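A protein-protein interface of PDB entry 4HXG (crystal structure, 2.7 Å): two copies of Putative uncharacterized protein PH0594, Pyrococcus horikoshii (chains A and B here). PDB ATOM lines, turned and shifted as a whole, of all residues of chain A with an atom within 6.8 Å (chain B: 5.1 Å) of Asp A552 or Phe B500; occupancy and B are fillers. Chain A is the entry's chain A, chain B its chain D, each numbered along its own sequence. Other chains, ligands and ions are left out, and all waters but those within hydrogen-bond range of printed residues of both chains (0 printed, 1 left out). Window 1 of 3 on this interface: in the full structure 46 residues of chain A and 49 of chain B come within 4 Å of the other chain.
Printed residues of chain B that touch a printed residue of chain A: Trp B140, Leu B495, Thr B496, Tyr B498, Ala B499, Phe B500 and Asp B552. Hydrophobic or aromatic side chains of chain B within 4 Å of the printed part of chain A: Trp B140, Leu B495, Tyr B498, Ala B499 and Phe B500.
The backbone carbonyl oxygen of Ala B499 sits at hydrogen-bond distance from a ring nitrogen (ND1) of His A559.
Thr A496 touches its own counterpart, Thr B496. Phe A500 touches Asp B552, and with the chains exchanged Asp A552 touches Phe B500. Positions printed for both chains: 496, 497, 500, 501, 550 and 552. Of the 13 pairs that touch across the chains among the printed residues, 3 have their exchanged pair printed and touching as well.
The backbone carbonyl oxygen (O) of Tyr A493 lies within hydrogen-bond range of the side-chain hydroxyl (OG1) of Thr A496 (3.3 Å). The side-chain hydroxyl (OG1) of Thr A496 sits at hydrogen-bond distance from the side-chain amide nitrogen (NE2) of Gln A553 (2.7 Å). The side-chain carboxylate (OD1) of Asp A552 lies within hydrogen-bond range of the side-chain hydroxyl (OG1) of Thr A496 (2.8 Å). The backbone carbonyl oxygen of Phe B500 sits at hydrogen-bond distance from the indole nitrogen of Trp B140, at 3.1 Å. OD1 of Asp B552 sits at hydrogen-bond distance from OG1 of Thr B496, 2.6 Å away. The side-chain amide oxygen (OE1) of Gln A553 sits at hydrogen-bond distance from the backbone NH (N) of Tyr A493 (3.0 Å).
Among the printed residues, merely in contact across the chains: Tyr A493 with Leu B495 (3.6 Å), Thr A496 with Thr B496 (3.6 Å), Phe A500 with Asp B552 (3.5 Å), Asp A552 with Phe B500 (3.7 Å), Leu A555 with Trp B140 (3.95 Å), Leu A555 with Phe B500 (3.4 Å), Met A556 with Thr B496 (3.8 Å), Met A556 with Ala B499 (3.7 Å), Met A556 with Phe B500 (3.9 Å), His A559 with Phe B500 (3.9 Å), Val A560 with Tyr B498 (3.9 Å) and Val A560 with Ala B499 (3.8 Å).
Of the printed residues of chain B, Tyr A493 touches Leu B495. Printed residues of chain B within 4 Å of Thr A496: Thr B496 (3.6 Å). Of the printed residues of chain B, Phe A500 touches Asp B552. Leu A528 touches none of the printed residues of chain B. Asp A552 touches one residue of chain B. Phe A557 touches none of the printed residues of chain B. Of the printed residues of chain A, Thr B496 touches Thr A496 and Met A556. Printed residues of chain A within 4 Å of Ala B499: Met A556, His A559 and Val A560. Printed residues of chain A within 4 Å of Phe B500: Asp A552, Leu A555, Met A556 and His A559. The nearest printed residue of chain B that does not touch Asp A552 is Thr B496 (5.5 Å).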
ATOM      1  N   GLY A 490      11.495  -7.573  -2.893  1.00  0.00           N
ATOM      2  CA  GLY A 490      10.607  -6.534  -2.402  1.00  0.00           C
ATOM      3  C   GLY A 490       9.230  -6.488  -3.037  1.00  0.00           C
ATOM      4  O   GLY A 490       8.753  -7.482  -3.598  1.00  0.00           O
ATOM      5  N   SER A 492       7.347  -3.699  -5.590  1.00  0.00           N
ATOM      6  CA  SER A 492       7.100  -2.447  -6.300  1.00  0.00           C
ATOM      7  C   SER A 492       5.643  -2.179  -6.691  1.00  0.00           C
ATOM      8  O   SER A 492       5.306  -1.063  -7.078  1.00  0.00           O
ATOM      9  CB  SER A 492       7.973  -2.374  -7.546  1.00  0.00           C
ATOM     10  OG  SER A 492       7.617  -3.405  -8.446  1.00  0.00           O
ATOM     11  N   TYR A 493       4.782  -3.190  -6.623  1.00  0.00           N
ATOM     12  CA  TYR A 493       3.364  -2.975  -6.924  1.00  0.00           C
ATOM     13  C   TYR A 493       2.451  -3.820  -6.040  1.00  0.00           C
ATOM     14  O   TYR A 493       2.513  -5.050  -6.074  1.00  0.00           O
ATOM     15  CB  TYR A 493       3.109  -3.284  -8.396  1.00  0.00           C
ATOM     16  CG  TYR A 493       1.757  -2.870  -8.905  1.00  0.00           C
ATOM     17  CD1 TYR A 493       0.860  -2.204  -8.091  1.00  0.00           C
ATOM     18  CD2 TYR A 493       1.375  -3.157 -10.210  1.00  0.00           C
ATOM     19  CE1 TYR A 493      -0.387  -1.827  -8.561  1.00  0.00           C
ATOM     20  CE2 TYR A 493       0.132  -2.784 -10.693  1.00  0.00           C
ATOM     21  CZ  TYR A 493      -0.748  -2.119  -9.864  1.00  0.00           C
ATOM     22  OH  TYR A 493      -1.988  -1.747 -10.338  1.00  0.00           O
ATOM     23  N   THR A 496      -0.416  -6.674  -7.647  1.00  0.00           N
ATOM     24  CA  THR A 496       0.077  -7.985  -8.035  1.00  0.00           C
ATOM     25  C   THR A 496       0.567  -8.736  -6.815  1.00  0.00           C
ATOM     26  O   THR A 496       0.552  -9.968  -6.803  1.00  0.00           O
ATOM     27  CB  THR A 496       1.227  -7.901  -9.040  1.00  0.00           C
ATOM     28  OG1 THR A 496       2.416  -7.458  -8.374  1.00  0.00           O
ATOM     29  CG2 THR A 496       0.883  -6.952 -10.165  1.00  0.00           C
ATOM     30  N   SER A 497       1.023  -8.013  -5.796  1.00  0.00           N
ATOM     31  CA  SER A 497       1.334  -8.681  -4.546  1.00  0.00           C
ATOM     32  C   SER A 497       0.063  -9.364  -4.066  1.00  0.00           C
ATOM     33  O   SER A 497       0.082 -10.533  -3.686  1.00  0.00           O
ATOM     34  CB  SER A 497       1.816  -7.703  -3.493  1.00  0.00           C
ATOM     35  OG  SER A 497       1.608  -8.248  -2.206  1.00  0.00           O
ATOM     36  N   PHE A 500      -0.978 -12.253  -6.939  1.00  0.00           N
ATOM     37  CA  PHE A 500       0.065 -13.221  -7.290  1.00  0.00           C
ATOM     38  C   PHE A 500       0.568 -14.012  -6.078  1.00  0.00           C
ATOM     39  O   PHE A 500       0.540 -15.241  -6.065  1.00  0.00           O
ATOM     40  CB  PHE A 500       1.228 -12.526  -7.994  1.00  0.00           C
ATOM     41  CG  PHE A 500       1.909 -13.366  -9.041  1.00  0.00           C
ATOM     42  CD1 PHE A 500       1.439 -14.628  -9.368  1.00  0.00           C
ATOM     43  CD2 PHE A 500       3.031 -12.891  -9.702  1.00  0.00           C
ATOM     44  CE1 PHE A 500       2.078 -15.398 -10.342  1.00  0.00           C
ATOM     45  CE2 PHE A 500       3.670 -13.657 -10.674  1.00  0.00           C
ATOM     46  CZ  PHE A 500       3.192 -14.911 -10.993  1.00  0.00           C
ATOM     47  N   SER A 501       1.078 -13.297  -5.081  1.00  0.00           N
ATOM     48  CA  SER A 501       1.859 -13.889  -3.992  1.00  0.00           C
ATOM     49  C   SER A 501       1.087 -14.918  -3.177  1.00  0.00           C
ATOM     50  O   SER A 501      -0.139 -14.978  -3.221  1.00  0.00           O
ATOM     51  CB  SER A 501       2.354 -12.790  -3.047  1.00  0.00           C
ATOM     52  OG  SER A 501       1.291 -12.291  -2.254  1.00  0.00           O
ATOM     53  N   LEU A 528       6.319   1.461  -8.078  1.00  0.00           N
ATOM     54  CA  LEU A 528       6.361   1.331  -9.534  1.00  0.00           C
ATOM     55  C   LEU A 528       5.906   2.599 -10.243  1.00  0.00           C
ATOM     56  O   LEU A 528       6.520   3.017 -11.223  1.00  0.00           O
ATOM     57  CB  LEU A 528       5.516   0.138 -10.009  1.00  0.00           C
ATOM     58  CG  LEU A 528       5.594  -0.162 -11.514  1.00  0.00           C
ATOM     59  CD1 LEU A 528       6.944  -0.753 -11.882  1.00  0.00           C
ATOM     60  CD2 LEU A 528       4.475  -1.087 -11.956  1.00  0.00           C
ATOM     61  N   HIS A 542      16.758 -10.884  -6.719  1.00  0.00           N
ATOM     62  CA  HIS A 542      15.581 -11.731  -6.583  1.00  0.00           C
ATOM     63  C   HIS A 542      15.913 -13.215  -6.733  1.00  0.00           C
ATOM     64  O   HIS A 542      16.980 -13.585  -7.241  1.00  0.00           O
ATOM     65  CB  HIS A 542      14.508 -11.320  -7.591  1.00  0.00           C
ATOM     66  CG  HIS A 542      13.108 -11.461  -7.074  1.00  0.00           C
ATOM     67  ND1 HIS A 542      12.427 -10.424  -6.474  1.00  0.00           N
ATOM     68  CD2 HIS A 542      12.266 -12.520  -7.058  1.00  0.00           C
ATOM     69  CE1 HIS A 542      11.225 -10.835  -6.115  1.00  0.00           C
ATOM     70  NE2 HIS A 542      11.103 -12.105  -6.457  1.00  0.00           N
ATOM     71  N   CYS A 549       7.120 -12.784  -2.354  1.00  0.00           N
ATOM     72  CA  CYS A 549       7.184 -11.632  -3.245  1.00  0.00           C
ATOM     73  C   CYS A 549       7.692 -12.107  -4.594  1.00  0.00           C
ATOM     74  O   CYS A 549       8.900 -12.166  -4.831  1.00  0.00           O
ATOM     75  CB  CYS A 549       8.082 -10.525  -2.676  1.00  0.00           C
ATOM     76  SG  CYS A 549       7.684 -10.039  -0.982  1.00  0.00           S
ATOM     77  N   PRO A 550       6.761 -12.455  -5.485  1.00  0.00           N
ATOM     78  CA  PRO A 550       7.050 -13.079  -6.773  1.00  0.00           C
ATOM     79  C   PRO A 550       7.992 -12.224  -7.611  1.00  0.00           C
ATOM     80  O   PRO A 550       8.136 -11.020  -7.384  1.00  0.00           O
ATOM     81  CB  PRO A 550       5.674 -13.158  -7.431  1.00  0.00           C
ATOM     82  CG  PRO A 550       4.732 -13.173  -6.304  1.00  0.00           C
ATOM     83  CD  PRO A 550       5.320 -12.255  -5.290  1.00  0.00           C
ATOM     84  N   LEU A 551       8.638 -12.871  -8.571  1.00  0.00           N
ATOM     85  CA  LEU A 551       9.688 -12.254  -9.358  1.00  0.00           C
ATOM     86  C   LEU A 551       9.268 -10.938 -10.021  1.00  0.00           C
ATOM     87  O   LEU A 551      10.106 -10.070 -10.264  1.00  0.00           O
ATOM     88  CB  LEU A 551      10.177 -13.241 -10.411  1.00  0.00           C
ATOM     89  CG  LEU A 551      11.134 -12.662 -11.444  1.00  0.00           C
ATOM     90  CD1 LEU A 551      12.507 -12.455 -10.822  1.00  0.00           C
ATOM     91  CD2 LEU A 551      11.205 -13.587 -12.641  1.00  0.00           C
ATOM     92  N   ASP A 552       7.977 -10.792 -10.314  1.00  0.00           N
ATOM     93  CA  ASP A 552       7.479  -9.593 -10.996  1.00  0.00           C
ATOM     94  C   ASP A 552       7.801  -8.289 -10.235  1.00  0.00           C
ATOM     95  O   ASP A 552       8.055  -7.242 -10.842  1.00  0.00           O
ATOM     96  CB  ASP A 552       5.971  -9.708 -11.241  1.00  0.00           C
ATOM     97  CG  ASP A 552       5.171  -9.759  -9.945  1.00  0.00           C
ATOM     98  OD1 ASP A 552       4.195  -8.995  -9.806  1.00  0.00           O
ATOM     99  OD2 ASP A 552       5.519 -10.564  -9.057  1.00  0.00           O
ATOM    100  N   GLN A 553       7.791  -8.366  -8.909  1.00  0.00           N
ATOM    101  CA  GLN A 553       8.010  -7.197  -8.065  1.00  0.00           C
ATOM    102  C   GLN A 553       9.344  -6.514  -8.354  1.00  0.00           C
ATOM    103  O   GLN A 553       9.431  -5.286  -8.332  1.00  0.00           O
ATOM    104  CB  GLN A 553       7.936  -7.588  -6.587  1.00  0.00           C
ATOM    105  CG  GLN A 553       6.599  -8.175  -6.178  1.00  0.00           C
ATOM    106  CD  GLN A 553       5.493  -7.146  -6.236  1.00  0.00           C
ATOM    107  OE1 GLN A 553       5.744  -5.943  -6.132  1.00  0.00           O
ATOM    108  NE2 GLN A 553       4.258  -7.611  -6.403  1.00  0.00           N
ATOM    109  N   SER A 554      10.389  -7.309  -8.564  1.00  0.00           N
ATOM    110  CA  SER A 554      11.693  -6.764  -8.916  1.00  0.00           C
ATOM    111  C   SER A 554      11.782  -6.448 -10.397  1.00  0.00           C
ATOM    112  O   SER A 554      12.277  -5.396 -10.789  1.00  0.00           O
ATOM    113  CB  SER A 554      12.804  -7.753  -8.553  1.00  0.00           C
ATOM    114  OG  SER A 554      12.742  -8.124  -7.192  1.00  0.00           O
ATOM    115  N   LEU A 555      11.288  -7.365 -11.218  1.00  0.00           N
ATOM    116  CA  LEU A 555      11.535  -7.294 -12.652  1.00  0.00           C
ATOM    117  C   LEU A 555      10.703  -6.203 -13.316  1.00  0.00           C
ATOM    118  O   LEU A 555      11.183  -5.515 -14.219  1.00  0.00           O
ATOM    119  CB  LEU A 555      11.282  -8.647 -13.321  1.00  0.00           C
ATOM    120  CG  LEU A 555      11.721  -8.791 -14.781  1.00  0.00           C
ATOM    121  CD1 LEU A 555      13.154  -8.308 -15.011  1.00  0.00           C
ATOM    122  CD2 LEU A 555      11.563 -10.236 -15.225  1.00  0.00           C
ATOM    123  N   MET A 556       9.462  -6.030 -12.870  1.00  0.00           N
ATOM    124  CA  MET A 556       8.637  -4.967 -13.427  1.00  0.00           C
ATOM    125  C   MET A 556       9.317  -3.634 -13.177  1.00  0.00           C
ATOM    126  O   MET A 556       9.405  -2.780 -14.073  1.00  0.00           O
ATOM    127  CB  MET A 556       7.233  -4.976 -12.825  1.00  0.00           C
ATOM    128  CG  MET A 556       6.402  -6.156 -13.286  1.00  0.00           C
ATOM    129  SD  MET A 556       4.654  -6.012 -12.897  1.00  0.00           S
ATOM    130  CE  MET A 556       4.711  -6.016 -11.114  1.00  0.00           C
ATOM    131  N   PHE A 557       9.824  -3.475 -11.958  1.00  0.00           N
ATOM    132  CA  PHE A 557      10.494  -2.248 -11.580  1.00  0.00           C
ATOM    133  C   PHE A 557      11.745  -2.088 -12.445  1.00  0.00           C
ATOM    134  O   PHE A 557      11.999  -1.010 -12.986  1.00  0.00           O
ATOM    135  CB  PHE A 557      10.845  -2.284 -10.095  1.00  0.00           C
ATOM    136  CG  PHE A 557      11.032  -0.928  -9.475  1.00  0.00           C
ATOM    137  CD1 PHE A 557      10.356   0.171  -9.959  1.00  0.00           C
ATOM    138  CD2 PHE A 557      11.891  -0.759  -8.405  1.00  0.00           C
ATOM    139  CE1 PHE A 557      10.532   1.415  -9.384  1.00  0.00           C
ATOM    140  CE2 PHE A 557      12.076   0.480  -7.829  1.00  0.00           C
ATOM    141  CZ  PHE A 557      11.394   1.568  -8.317  1.00  0.00           C
ATOM    142  N   TYR A 558      12.507  -3.170 -12.603  1.00  0.00           N
ATOM    143  CA  TYR A 558      13.708  -3.122 -13.432  1.00  0.00           C
ATOM    144  C   TYR A 558      13.407  -2.707 -14.879  1.00  0.00           C
ATOM    145  O   TYR A 558      14.092  -1.839 -15.416  1.00  0.00           O
ATOM    146  CB  TYR A 558      14.489  -4.444 -13.403  1.00  0.00           C
ATOM    147  CG  TYR A 558      15.648  -4.457 -14.382  1.00  0.00           C
ATOM    148  CD1 TYR A 558      16.860  -3.846 -14.071  1.00  0.00           C
ATOM    149  CD2 TYR A 558      15.521  -5.056 -15.631  1.00  0.00           C
ATOM    150  CE1 TYR A 558      17.915  -3.844 -14.977  1.00  0.00           C
ATOM    151  CE2 TYR A 558      16.562  -5.057 -16.537  1.00  0.00           C
ATOM    152  CZ  TYR A 558      17.755  -4.453 -16.210  1.00  0.00           C
ATOM    153  OH  TYR A 558      18.782  -4.458 -17.126  1.00  0.00           O
ATOM    154  N   HIS A 559      12.395  -3.309 -15.510  1.00  0.00           N
ATOM    155  CA  HIS A 559      12.077  -2.972 -16.904  1.00  0.00           C
ATOM    156  C   HIS A 559      11.624  -1.516 -17.027  1.00  0.00           C
ATOM    157  O   HIS A 559      12.129  -0.758 -17.877  1.00  0.00           O
ATOM    158  CB  HIS A 559      11.003  -3.902 -17.492  1.00  0.00           C
ATOM    159  CG  HIS A 559      11.522  -5.233 -17.934  1.00  0.00           C
ATOM    160  ND1 HIS A 559      10.736  -6.364 -17.970  1.00  0.00           N
ATOM    161  CD2 HIS A 559      12.751  -5.617 -18.359  1.00  0.00           C
ATOM    162  CE1 HIS A 559      11.457  -7.387 -18.394  1.00  0.00           C
ATOM    163  NE2 HIS A 559      12.683  -6.960 -18.637  1.00  0.00           N
ATOM    164  N   VAL A 560      10.663  -1.134 -16.189  1.00  0.00           N
ATOM    165  CA  VAL A 560      10.127   0.218 -16.237  1.00  0.00           C
ATOM    166  C   VAL A 560      11.224   1.269 -16.035  1.00  0.00           C
ATOM    167  O   VAL A 560      11.229   2.307 -16.699  1.00  0.00           O
ATOM    168  CB  VAL A 560       9.024   0.411 -15.206  1.00  0.00           C
ATOM    169  CG1 VAL A 560       8.557   1.848 -15.201  1.00  0.00           C
ATOM    170  CG2 VAL A 560       7.866  -0.522 -15.510  1.00  0.00           C
ATOM    171  N   TRP B 140      14.363 -11.217 -20.444  1.00  0.00           N
ATOM    172  CA  TRP B 140      14.119 -12.534 -21.023  1.00  0.00           C
ATOM    173  C   TRP B 140      13.351 -12.471 -22.338  1.00  0.00           C
ATOM    174  O   TRP B 140      12.735 -11.454 -22.675  1.00  0.00           O
ATOM    175  CB  TRP B 140      13.366 -13.428 -20.034  1.00  0.00           C
ATOM    176  CG  TRP B 140      12.065 -12.840 -19.538  1.00  0.00           C
ATOM    177  CD1 TRP B 140      11.397 -11.766 -20.048  1.00  0.00           C
ATOM    178  CD2 TRP B 140      11.295 -13.294 -18.422  1.00  0.00           C
ATOM    179  NE1 TRP B 140      10.255 -11.529 -19.323  1.00  0.00           N
ATOM    180  CE2 TRP B 140      10.173 -12.452 -18.317  1.00  0.00           C
ATOM    181  CE3 TRP B 140      11.450 -14.332 -17.501  1.00  0.00           C
ATOM    182  CZ2 TRP B 140       9.213 -12.614 -17.332  1.00  0.00           C
ATOM    183  CZ3 TRP B 140      10.502 -14.494 -16.527  1.00  0.00           C
ATOM    184  CH2 TRP B 140       9.393 -13.642 -16.447  1.00  0.00           C
ATOM    185  N   LEU B 495      -1.185  -3.939 -17.651  1.00  0.00           N
ATOM    186  CA  LEU B 495      -0.066  -3.253 -17.027  1.00  0.00           C
ATOM    187  C   LEU B 495       1.097  -4.208 -16.829  1.00  0.00           C
ATOM    188  O   LEU B 495       2.225  -3.900 -17.217  1.00  0.00           O
ATOM    189  CB  LEU B 495      -0.473  -2.639 -15.694  1.00  0.00           C
ATOM    190  CG  LEU B 495       0.529  -1.633 -15.128  1.00  0.00           C
ATOM    191  CD1 LEU B 495       0.822  -0.551 -16.153  1.00  0.00           C
ATOM    192  CD2 LEU B 495      -0.008  -1.026 -13.844  1.00  0.00           C
ATOM    193  N   THR B 496       0.830  -5.368 -16.232  1.00  0.00           N
ATOM    194  CA  THR B 496       1.896  -6.330 -16.011  1.00  0.00           C
ATOM    195  C   THR B 496       2.377  -6.918 -17.328  1.00  0.00           C
ATOM    196  O   THR B 496       3.537  -7.301 -17.439  1.00  0.00           O
ATOM    197  CB  THR B 496       1.528  -7.447 -15.016  1.00  0.00           C
ATOM    198  OG1 THR B 496       0.558  -8.316 -15.602  1.00  0.00           O
ATOM    199  CG2 THR B 496       0.992  -6.863 -13.715  1.00  0.00           C
ATOM    200  N   SER B 497       1.512  -6.984 -18.335  1.00  0.00           N
ATOM    201  CA  SER B 497       2.002  -7.381 -19.648  1.00  0.00           C
ATOM    202  C   SER B 497       3.134  -6.443 -20.071  1.00  0.00           C
ATOM    203  O   SER B 497       4.210  -6.890 -20.492  1.00  0.00           O
ATOM    204  CB  SER B 497       0.900  -7.333 -20.697  1.00  0.00           C
ATOM    205  OG  SER B 497       1.471  -7.298 -21.998  1.00  0.00           O
ATOM    206  N   TYR B 498       2.885  -5.142 -19.943  1.00  0.00           N
ATOM    207  CA  TYR B 498       3.848  -4.121 -20.340  1.00  0.00           C
ATOM    208  C   TYR B 498       5.180  -4.160 -19.572  1.00  0.00           C
ATOM    209  O   TYR B 498       6.252  -4.059 -20.175  1.00  0.00           O
ATOM    210  CB  TYR B 498       3.209  -2.740 -20.202  1.00  0.00           C
ATOM    211  CG  TYR B 498       4.207  -1.640 -19.958  1.00  0.00           C
ATOM    212  CD1 TYR B 498       4.977  -1.135 -20.996  1.00  0.00           C
ATOM    213  CD2 TYR B 498       4.394  -1.117 -18.686  1.00  0.00           C
ATOM    214  CE1 TYR B 498       5.901  -0.135 -20.776  1.00  0.00           C
ATOM    215  CE2 TYR B 498       5.316  -0.114 -18.459  1.00  0.00           C
ATOM    216  CZ  TYR B 498       6.067   0.369 -19.510  1.00  0.00           C
ATOM    217  OH  TYR B 498       6.992   1.364 -19.300  1.00  0.00           O
ATOM    218  N   ALA B 499       5.105  -4.267 -18.246  1.00  0.00           N
ATOM    219  CA  ALA B 499       6.295  -4.233 -17.383  1.00  0.00           C
ATOM    220  C   ALA B 499       7.062  -5.552 -17.269  1.00  0.00           C
ATOM    221  O   ALA B 499       8.282  -5.565 -17.207  1.00  0.00           O
ATOM    222  CB  ALA B 499       5.913  -3.747 -16.002  1.00  0.00           C
ATOM    223  N   PHE B 500       6.315  -6.641 -17.139  1.00  0.00           N
ATOM    224  CA  PHE B 500       6.842  -7.994 -16.946  1.00  0.00           C
ATOM    225  C   PHE B 500       7.266  -8.773 -18.209  1.00  0.00           C
ATOM    226  O   PHE B 500       8.224  -9.541 -18.175  1.00  0.00           O
ATOM    227  CB  PHE B 500       5.826  -8.812 -16.147  1.00  0.00           C
ATOM    228  CG  PHE B 500       6.425  -9.923 -15.352  1.00  0.00           C
ATOM    229  CD1 PHE B 500       7.785  -9.971 -15.110  1.00  0.00           C
ATOM    230  CD2 PHE B 500       5.623 -10.932 -14.847  1.00  0.00           C
ATOM    231  CE1 PHE B 500       8.338 -11.003 -14.372  1.00  0.00           C
ATOM    232  CE2 PHE B 500       6.167 -11.965 -14.107  1.00  0.00           C
ATOM    233  CZ  PHE B 500       7.530 -11.999 -13.871  1.00  0.00           C
ATOM    234  N   SER B 501       6.512  -8.626 -19.297  1.00  0.00           N
ATOM    235  CA  SER B 501       6.685  -9.495 -20.470  1.00  0.00           C
ATOM    236  C   SER B 501       7.855  -9.140 -21.369  1.00  0.00           C
ATOM    237  O   SER B 501       8.280  -7.990 -21.444  1.00  0.00           O
ATOM    238  CB  SER B 501       5.414  -9.546 -21.321  1.00  0.00           C
ATOM    239  OG  SER B 501       5.465  -8.585 -22.356  1.00  0.00           O
ATOM    240  N   ASP B 502       8.343 -10.143 -22.086  1.00  0.00           N
ATOM    241  CA  ASP B 502       9.476  -9.959 -22.979  1.00  0.00           C
ATOM    242  C   ASP B 502       9.324  -8.792 -23.972  1.00  0.00           C
ATOM    243  O   ASP B 502      10.255  -7.994 -24.131  1.00  0.00           O
ATOM    244  CB  ASP B 502       9.825 -11.275 -23.693  1.00  0.00           C
ATOM    245  CG  ASP B 502       8.769 -11.709 -24.694  1.00  0.00           C
ATOM    246  OD1 ASP B 502       7.654 -11.148 -24.688  1.00  0.00           O
ATOM    247  OD2 ASP B 502       9.062 -12.632 -25.485  1.00  0.00           O
ATOM    248  N   PRO B 550       3.506 -13.789 -19.307  1.00  0.00           N
ATOM    249  CA  PRO B 550       4.068 -14.357 -18.075  1.00  0.00           C
ATOM    250  C   PRO B 550       3.000 -14.962 -17.172  1.00  0.00           C
ATOM    251  O   PRO B 550       1.824 -14.650 -17.317  1.00  0.00           O
ATOM    252  CB  PRO B 550       4.735 -13.153 -17.414  1.00  0.00           C
ATOM    253  CG  PRO B 550       5.091 -12.251 -18.575  1.00  0.00           C
ATOM    254  CD  PRO B 550       3.948 -12.402 -19.536  1.00  0.00           C
ATOM    255  N   ASP B 552       1.794 -14.632 -14.204  1.00  0.00           N
ATOM    256  CA  ASP B 552       0.862 -13.837 -13.395  1.00  0.00           C
ATOM    257  C   ASP B 552      -0.480 -13.669 -14.108  1.00  0.00           C
ATOM    258  O   ASP B 552      -1.537 -13.642 -13.474  1.00  0.00           O
ATOM    259  CB  ASP B 552       1.445 -12.464 -13.080  1.00  0.00           C
ATOM    260  CG  ASP B 552       1.734 -11.666 -14.331  1.00  0.00           C
ATOM    261  OD1 ASP B 552       1.269 -10.509 -14.437  1.00  0.00           O
ATOM    262  OD2 ASP B 552       2.423 -12.211 -15.220  1.00  0.00           O
